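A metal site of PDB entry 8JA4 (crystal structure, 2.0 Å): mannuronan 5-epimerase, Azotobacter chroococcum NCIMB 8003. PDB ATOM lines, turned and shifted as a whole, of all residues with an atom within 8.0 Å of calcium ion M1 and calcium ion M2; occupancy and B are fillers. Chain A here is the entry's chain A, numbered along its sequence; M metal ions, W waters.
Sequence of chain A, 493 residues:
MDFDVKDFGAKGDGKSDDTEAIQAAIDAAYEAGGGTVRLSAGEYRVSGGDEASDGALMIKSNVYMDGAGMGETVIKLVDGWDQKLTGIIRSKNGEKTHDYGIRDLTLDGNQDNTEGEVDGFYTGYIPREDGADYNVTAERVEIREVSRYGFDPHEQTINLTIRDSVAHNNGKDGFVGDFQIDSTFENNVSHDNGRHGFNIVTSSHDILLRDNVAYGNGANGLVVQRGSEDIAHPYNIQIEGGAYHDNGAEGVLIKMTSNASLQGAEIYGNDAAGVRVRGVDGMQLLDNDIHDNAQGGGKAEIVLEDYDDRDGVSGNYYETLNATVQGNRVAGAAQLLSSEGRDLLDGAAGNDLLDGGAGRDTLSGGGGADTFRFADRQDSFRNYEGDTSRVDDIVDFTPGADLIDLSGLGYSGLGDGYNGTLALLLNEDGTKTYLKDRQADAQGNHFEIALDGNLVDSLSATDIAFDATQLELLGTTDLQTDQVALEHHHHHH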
ATOM      1  N   VAL A 330      14.871  -2.685  -5.421  1.00  0.00           N
ATOM      2  CA  VAL A 330      15.023  -1.318  -4.931  1.00  0.00           C
ATOM      3  C   VAL A 330      13.702  -0.596  -5.041  1.00  0.00           C
ATOM      4  O   VAL A 330      13.307  -0.167  -6.138  1.00  0.00           O
ATOM      5  CB  VAL A 330      16.097  -0.526  -5.691  1.00  0.00           C
ATOM      6  CG1 VAL A 330      16.230   0.874  -5.083  1.00  0.00           C
ATOM      7  CG2 VAL A 330      17.441  -1.261  -5.640  1.00  0.00           C
ATOM      8  N   GLY A 332      12.283   2.315  -4.841  1.00  0.00           N
ATOM      9  CA  GLY A 332      12.498   3.747  -4.846  1.00  0.00           C
ATOM     10  C   GLY A 332      13.676   4.107  -5.750  1.00  0.00           C
ATOM     11  O   GLY A 332      14.253   3.274  -6.427  1.00  0.00           O
ATOM     12  N   ALA A 333      14.006   5.376  -5.747  1.00  0.00           N
ATOM     13  CA  ALA A 333      14.879   5.898  -6.805  1.00  0.00           C
ATOM     14  C   ALA A 333      16.341   5.506  -6.572  1.00  0.00           C
ATOM     15  O   ALA A 333      16.876   5.611  -5.450  1.00  0.00           O
ATOM     16  CB  ALA A 333      14.758   7.411  -6.851  1.00  0.00           C
ATOM     17  N   ALA A 334      17.029   5.100  -7.638  1.00  0.00           N
ATOM     18  CA  ALA A 334      18.484   4.930  -7.560  1.00  0.00           C
ATOM     19  C   ALA A 334      19.198   6.018  -8.364  1.00  0.00           C
ATOM     20  O   ALA A 334      18.855   6.269  -9.532  1.00  0.00           O
ATOM     21  CB  ALA A 334      18.889   3.530  -8.032  1.00  0.00           C
ATOM     22  N   ASP A 346      22.533  -0.950 -13.345  1.00  0.00           N
ATOM     23  CA  ASP A 346      21.142  -1.394 -13.507  1.00  0.00           C
ATOM     24  C   ASP A 346      20.286  -0.739 -12.441  1.00  0.00           C
ATOM     25  O   ASP A 346      20.507  -0.958 -11.246  1.00  0.00           O
ATOM     26  CB  ASP A 346      21.027  -2.907 -13.356  1.00  0.00           C
ATOM     27  CG  ASP A 346      21.709  -3.697 -14.474  1.00  0.00           C
ATOM     28  OD1 ASP A 346      22.048  -3.113 -15.534  1.00  0.00           O
ATOM     29  OD2 ASP A 346      21.888  -4.927 -14.282  1.00  0.00           O
ATOM     30  N   GLY A 347      19.276   0.023 -12.870  1.00  0.00           N
ATOM     31  CA  GLY A 347      18.200   0.434 -11.990  1.00  0.00           C
ATOM     32  C   GLY A 347      17.230  -0.716 -11.667  1.00  0.00           C
ATOM     33  O   GLY A 347      17.395  -1.868 -12.072  1.00  0.00           O
ATOM     34  N   ALA A 348      16.172  -0.368 -10.917  1.00  0.00           N
ATOM     35  CA  ALA A 348      15.245  -1.329 -10.346  1.00  0.00           C
ATOM     36  C   ALA A 348      13.884  -0.690 -10.492  1.00  0.00           C
ATOM     37  O   ALA A 348      13.690   0.101 -11.426  1.00  0.00           O
ATOM     38  CB  ALA A 348      15.592  -1.670  -8.898  1.00  0.00           C
ATOM     39  N   ALA A 349      12.919  -1.036  -9.634  1.00  0.00           N
ATOM     40  CA  ALA A 349      11.530  -0.617  -9.867  1.00  0.00           C
ATOM     41  C   ALA A 349      11.300   0.883  -9.726  1.00  0.00           C
ATOM     42  O   ALA A 349      10.217   1.348 -10.105  1.00  0.00           O
ATOM     43  CB  ALA A 349      10.593  -1.354  -8.895  1.00  0.00           C
ATOM     44  N   GLY A 350      12.268   1.649  -9.195  1.00  0.00           N
ATOM     45  CA  GLY A 350      12.130   3.088  -9.036  1.00  0.00           C
ATOM     46  C   GLY A 350      12.361   3.891 -10.322  1.00  0.00           C
ATOM     47  O   GLY A 350      12.694   3.354 -11.377  1.00  0.00           O
ATOM     48  N   ASN A 351      12.121   5.194 -10.228  1.00  0.00           N
ATOM     49  CA  ASN A 351      12.389   6.144 -11.314  1.00  0.00           C
ATOM     50  C   ASN A 351      13.830   6.594 -11.129  1.00  0.00           C
ATOM     51  O   ASN A 351      14.122   7.469 -10.317  1.00  0.00           O
ATOM     52  CB  ASN A 351      11.436   7.330 -11.251  1.00  0.00           C
ATOM     53  CG  ASN A 351       9.996   6.995 -11.599  1.00  0.00           C
ATOM     54  OD1 ASN A 351       9.650   5.899 -12.059  1.00  0.00           O
ATOM     55  ND2 ASN A 351       9.144   7.966 -11.349  1.00  0.00           N
ATOM     56  N   ASP A 352      14.754   5.961 -11.844  1.00  0.00           N
ATOM     57  CA  ASP A 352      16.177   6.094 -11.571  1.00  0.00           C
ATOM     58  C   ASP A 352      16.870   7.066 -12.511  1.00  0.00           C
ATOM     59  O   ASP A 352      16.426   7.348 -13.629  1.00  0.00           O
ATOM     60  CB  ASP A 352      16.844   4.720 -11.679  1.00  0.00           C
ATOM     61  CG  ASP A 352      16.086   3.631 -10.885  1.00  0.00           C
ATOM     62  OD1 ASP A 352      15.809   3.789  -9.659  1.00  0.00           O
ATOM     63  OD2 ASP A 352      15.775   2.594 -11.493  1.00  0.00           O
ATOM     64  N   LEU A 353      18.017   7.560 -12.063  1.00  0.00           N
ATOM     65  CA  LEU A 353      18.878   8.400 -12.873  1.00  0.00           C
ATOM     66  C   LEU A 353      20.171   7.636 -13.128  1.00  0.00           C
ATOM     67  O   LEU A 353      20.891   7.298 -12.164  1.00  0.00           O
ATOM     68  CB  LEU A 353      19.174   9.723 -12.157  1.00  0.00           C
ATOM     69  CG  LEU A 353      20.272  10.585 -12.788  1.00  0.00           C
ATOM     70  CD1 LEU A 353      19.761  10.992 -14.148  1.00  0.00           C
ATOM     71  CD2 LEU A 353      20.540  11.847 -11.951  1.00  0.00           C
ATOM     72  N   LEU A 354      20.501   7.395 -14.399  1.00  0.00           N
ATOM     73  CA  LEU A 354      21.691   6.631 -14.778  1.00  0.00           C
ATOM     74  C   LEU A 354      22.619   7.458 -15.637  1.00  0.00           C
ATOM     75  O   LEU A 354      22.173   8.036 -16.641  1.00  0.00           O
ATOM     76  CB  LEU A 354      21.298   5.356 -15.531  1.00  0.00           C
ATOM     77  CG  LEU A 354      20.573   4.395 -14.630  1.00  0.00           C
ATOM     78  CD1 LEU A 354      19.090   4.578 -14.862  1.00  0.00           C
ATOM     79  CD2 LEU A 354      21.043   3.033 -15.067  1.00  0.00           C
ATOM     80  N   SER A 364      20.821  -0.091 -17.635  1.00  0.00           N
ATOM     81  CA  SER A 364      19.436  -0.530 -17.786  1.00  0.00           C
ATOM     82  C   SER A 364      18.601   0.095 -16.692  1.00  0.00           C
ATOM     83  O   SER A 364      19.096   0.317 -15.583  1.00  0.00           O
ATOM     84  CB  SER A 364      19.348  -2.049 -17.769  1.00  0.00           C
ATOM     85  OG  SER A 364      19.326  -2.504 -16.448  1.00  0.00           O
ATOM     86  N   GLY A 365      17.364   0.475 -17.017  1.00  0.00           N
ATOM     87  CA  GLY A 365      16.563   1.165 -16.032  1.00  0.00           C
ATOM     88  C   GLY A 365      15.656   0.273 -15.199  1.00  0.00           C
ATOM     89  O   GLY A 365      15.245   0.640 -14.079  1.00  0.00           O
ATOM     90  N   GLY A 366      15.307  -0.888 -15.742  1.00  0.00           N
ATOM     91  CA  GLY A 366      14.259  -1.678 -15.075  1.00  0.00           C
ATOM     92  C   GLY A 366      12.914  -0.971 -15.156  1.00  0.00           C
ATOM     93  O   GLY A 366      12.675  -0.100 -16.023  1.00  0.00           O
ATOM     94  N   GLY A 367      12.014  -1.348 -14.226  1.00  0.00           N
ATOM     95  CA  GLY A 367      10.662  -0.804 -14.230  1.00  0.00           C
ATOM     96  C   GLY A 367      10.675   0.662 -13.837  1.00  0.00           C
ATOM     97  O   GLY A 367      11.720   1.246 -13.563  1.00  0.00           O
ATOM     98  N   GLY A 368       9.507   1.318 -13.889  1.00  0.00           N
ATOM     99  CA  GLY A 368       9.471   2.760 -13.657  1.00  0.00           C
ATOM    100  C   GLY A 368      10.007   3.565 -14.836  1.00  0.00           C
ATOM    101  O   GLY A 368      10.417   3.040 -15.869  1.00  0.00           O
ATOM    102  N   ALA A 369      10.033   4.884 -14.679  1.00  0.00           N
ATOM    103  CA  ALA A 369      10.464   5.781 -15.753  1.00  0.00           C
ATOM    104  C   ALA A 369      11.849   6.304 -15.397  1.00  0.00           C
ATOM    105  O   ALA A 369      12.015   7.038 -14.419  1.00  0.00           O
ATOM    106  CB  ALA A 369       9.494   6.955 -15.927  1.00  0.00           C
ATOM    107  N   ASP A 370      12.846   5.932 -16.198  1.00  0.00           N
ATOM    108  CA  ASP A 370      14.230   6.218 -15.867  1.00  0.00           C
ATOM    109  C   ASP A 370      14.837   7.219 -16.850  1.00  0.00           C
ATOM    110  O   ASP A 370      14.486   7.265 -18.036  1.00  0.00           O
ATOM    111  CB  ASP A 370      15.068   4.934 -15.866  1.00  0.00           C
ATOM    112  CG  ASP A 370      14.430   3.835 -15.012  1.00  0.00           C
ATOM    113  OD1 ASP A 370      13.980   2.842 -15.564  1.00  0.00           O
ATOM    114  OD2 ASP A 370      14.394   3.945 -13.795  1.00  0.00           O
ATOM    115  N   THR A 371      15.771   8.004 -16.335  1.00  0.00           N
ATOM    116  CA  THR A 371      16.494   8.985 -17.132  1.00  0.00           C
ATOM    117  C   THR A 371      17.928   8.516 -17.317  1.00  0.00           C
ATOM    118  O   THR A 371      18.665   8.335 -16.337  1.00  0.00           O
ATOM    119  CB  THR A 371      16.438  10.356 -16.468  1.00  0.00           C
ATOM    120  OG1 THR A 371      15.061  10.787 -16.401  1.00  0.00           O
ATOM    121  CG2 THR A 371      17.210  11.344 -17.277  1.00  0.00           C
ATOM    122  N   PHE A 372      18.298   8.262 -18.578  1.00  0.00           N
ATOM    123  CA  PHE A 372      19.683   7.939 -18.913  1.00  0.00           C
ATOM    124  C   PHE A 372      20.339   9.232 -19.386  1.00  0.00           C
ATOM    125  O   PHE A 372      20.046   9.725 -20.489  1.00  0.00           O
ATOM    126  CB  PHE A 372      19.722   6.881 -20.000  1.00  0.00           C
ATOM    127  CG  PHE A 372      18.960   5.634 -19.679  1.00  0.00           C
ATOM    128  CD1 PHE A 372      19.605   4.526 -19.113  1.00  0.00           C
ATOM    129  CD2 PHE A 372      17.593   5.542 -19.958  1.00  0.00           C
ATOM    130  CE1 PHE A 372      18.897   3.359 -18.849  1.00  0.00           C
ATOM    131  CE2 PHE A 372      16.889   4.388 -19.694  1.00  0.00           C
ATOM    132  CZ  PHE A 372      17.540   3.286 -19.133  1.00  0.00           C
ATOM    133  N   ASP A 396      17.368  -1.668 -22.073  1.00  0.00           N
ATOM    134  CA  ASP A 396      15.916  -1.837 -22.029  1.00  0.00           C
ATOM    135  C   ASP A 396      15.198  -0.522 -22.188  1.00  0.00           C
ATOM    136  O   ASP A 396      14.223  -0.258 -21.489  1.00  0.00           O
ATOM    137  CB  ASP A 396      15.480  -2.456 -20.703  1.00  0.00           C
ATOM    138  CG  ASP A 396      15.862  -1.560 -19.482  1.00  0.00           C
ATOM    139  OD1 ASP A 396      16.698  -0.609 -19.618  1.00  0.00           O
ATOM    140  OD2 ASP A 396      15.322  -1.774 -18.388  1.00  0.00           O
ATOM    141  N   PHE A 397      15.659   0.353 -23.079  1.00  0.00           N
ATOM    142  CA  PHE A 397      14.973   1.628 -23.193  1.00  0.00           C
ATOM    143  C   PHE A 397      13.535   1.414 -23.630  1.00  0.00           C
ATOM    144  O   PHE A 397      13.268   0.682 -24.571  1.00  0.00           O
ATOM    145  CB  PHE A 397      15.667   2.556 -24.175  1.00  0.00           C
ATOM    146  CG  PHE A 397      15.137   3.961 -24.122  1.00  0.00           C
ATOM    147  CD1 PHE A 397      14.116   4.366 -24.984  1.00  0.00           C
ATOM    148  CD2 PHE A 397      15.645   4.883 -23.216  1.00  0.00           C
ATOM    149  CE1 PHE A 397      13.624   5.662 -24.929  1.00  0.00           C
ATOM    150  CE2 PHE A 397      15.161   6.177 -23.156  1.00  0.00           C
ATOM    151  CZ  PHE A 397      14.129   6.563 -24.030  1.00  0.00           C
ATOM    152  N   THR A 398      12.614   2.099 -22.949  1.00  0.00           N
ATOM    153  CA  THR A 398      11.172   1.864 -23.097  1.00  0.00           C
ATOM    154  C   THR A 398      10.511   3.154 -23.570  1.00  0.00           C
ATOM    155  O   THR A 398      10.354   4.101 -22.785  1.00  0.00           O
ATOM    156  CB  THR A 398      10.594   1.403 -21.762  1.00  0.00           C
ATOM    157  OG1 THR A 398      11.407   0.353 -21.228  1.00  0.00           O
ATOM    158  CG2 THR A 398       9.182   0.892 -21.927  1.00  0.00           C
ATOM    159  N   ALA A 401       8.059   5.882 -21.587  1.00  0.00           N
ATOM    160  CA  ALA A 401       8.330   5.894 -20.149  1.00  0.00           C
ATOM    161  C   ALA A 401       9.713   6.456 -19.826  1.00  0.00           C
ATOM    162  O   ALA A 401       9.860   7.401 -19.043  1.00  0.00           O
ATOM    163  CB  ALA A 401       8.190   4.468 -19.573  1.00  0.00           C
ATOM    164  N   ASP A 402      10.760   5.869 -20.404  1.00  0.00           N
ATOM    165  CA  ASP A 402      12.098   6.334 -20.118  1.00  0.00           C
ATOM    166  C   ASP A 402      12.409   7.620 -20.900  1.00  0.00           C
ATOM    167  O   ASP A 402      11.684   8.019 -21.827  1.00  0.00           O
ATOM    168  CB  ASP A 402      13.098   5.244 -20.456  1.00  0.00           C
ATOM    169  CG  ASP A 402      12.897   3.989 -19.654  1.00  0.00           C
ATOM    170  OD1 ASP A 402      12.520   4.068 -18.434  1.00  0.00           O
ATOM    171  OD2 ASP A 402      13.136   2.914 -20.255  1.00  0.00           O
ATOM    172  N   LEU A 403      13.542   8.240 -20.534  1.00  0.00           N
ATOM    173  CA  LEU A 403      14.013   9.470 -21.154  1.00  0.00           C
ATOM    174  C   LEU A 403      15.514   9.396 -21.369  1.00  0.00           C
ATOM    175  O   LEU A 403      16.243   8.938 -20.496  1.00  0.00           O
ATOM    176  CB  LEU A 403      13.715  10.706 -20.280  1.00  0.00           C
ATOM    177  CG  LEU A 403      14.165  12.076 -20.837  1.00  0.00           C
ATOM    178  CD1 LEU A 403      13.304  12.547 -22.025  1.00  0.00           C
ATOM    179  CD2 LEU A 403      14.085  13.094 -19.710  1.00  0.00           C
ATOM    180  N   THR A 476      12.162  12.442 -15.688  1.00  0.00           N
ATOM    181  CA  THR A 476      11.380  11.423 -15.007  1.00  0.00           C
ATOM    182  C   THR A 476      11.691  11.287 -13.517  1.00  0.00           C
ATOM    183  O   THR A 476      11.050  10.489 -12.821  1.00  0.00           O
ATOM    184  CB  THR A 476      11.577  10.065 -15.668  1.00  0.00           C
ATOM    185  OG1 THR A 476      12.851   9.516 -15.280  1.00  0.00           O
ATOM    186  CG2 THR A 476      11.466  10.211 -17.169  1.00  0.00           C
HETATM  187 CA    CA M   1      12.356   1.977 -17.075  1.00  0.00          CA
HETATM  188 CA    CA M   2      13.946   1.925 -12.831  1.00  0.00          CA
HETATM  189  O   HOH W   1      10.395   0.913 -18.416  1.00  0.00           O
HETATM  190  O   HOH W   2      14.228   1.192 -18.704  1.00  0.00           O
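OD2 of Asp 402 lies within hydrogen-bond range of N of Thr 398. N of Ala 334 sits at hydrogen-bond distance from OD1 of Asp 352, 2.7 Å away. The backbone carbonyl oxygen (O) of Asp 370 lies within hydrogen-bond range of the backbone NH (N) of Leu 403 (2.8 Å). The backbone NH of Thr 371 is in hydrogen-bond range of the backbone carbonyl oxygen of Asp 352, at 2.9 Å. N of Gly 366 lies within hydrogen-bond range of OD2 of Asp 396. The side-chain carboxylate (OD1) of Asp 396 sits at hydrogen-bond distance from the backbone NH (N) of Gly 365 (2.9 Å).
Of the 29 residues printed, 5 come within 4 Å of calcium ion M1.
Within 4 Å of calcium ion M2: Ala 348, Gly 350, Asp 352, Gly 365, Gly 366, Gly 367 and Asp 370.
Calcium ion M1 is bound by the backbone carbonyl oxygen of Gly 366, the side-chain carboxylate of Asp 370, the side-chain carboxylate of Asp 402, the backbone carbonyl oxygen of Gly 368, water W2 and water W1. Calcium ion M1 has six donor atoms within binding distance.
Calcium ion M2 is bound by O of Gly 365, OD2 of Asp 370, O of Ala 348, OD2 of Asp 352, O of Gly 350, O of Gly 367 and OD1 of Asp 370. Calcium ion M2 has seven donor atoms within binding distance.
Water W2 lies within hydrogen-bond range of OD2 of Asp 402 (2.6 Å) and O of Asp 396 (3.1 Å).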
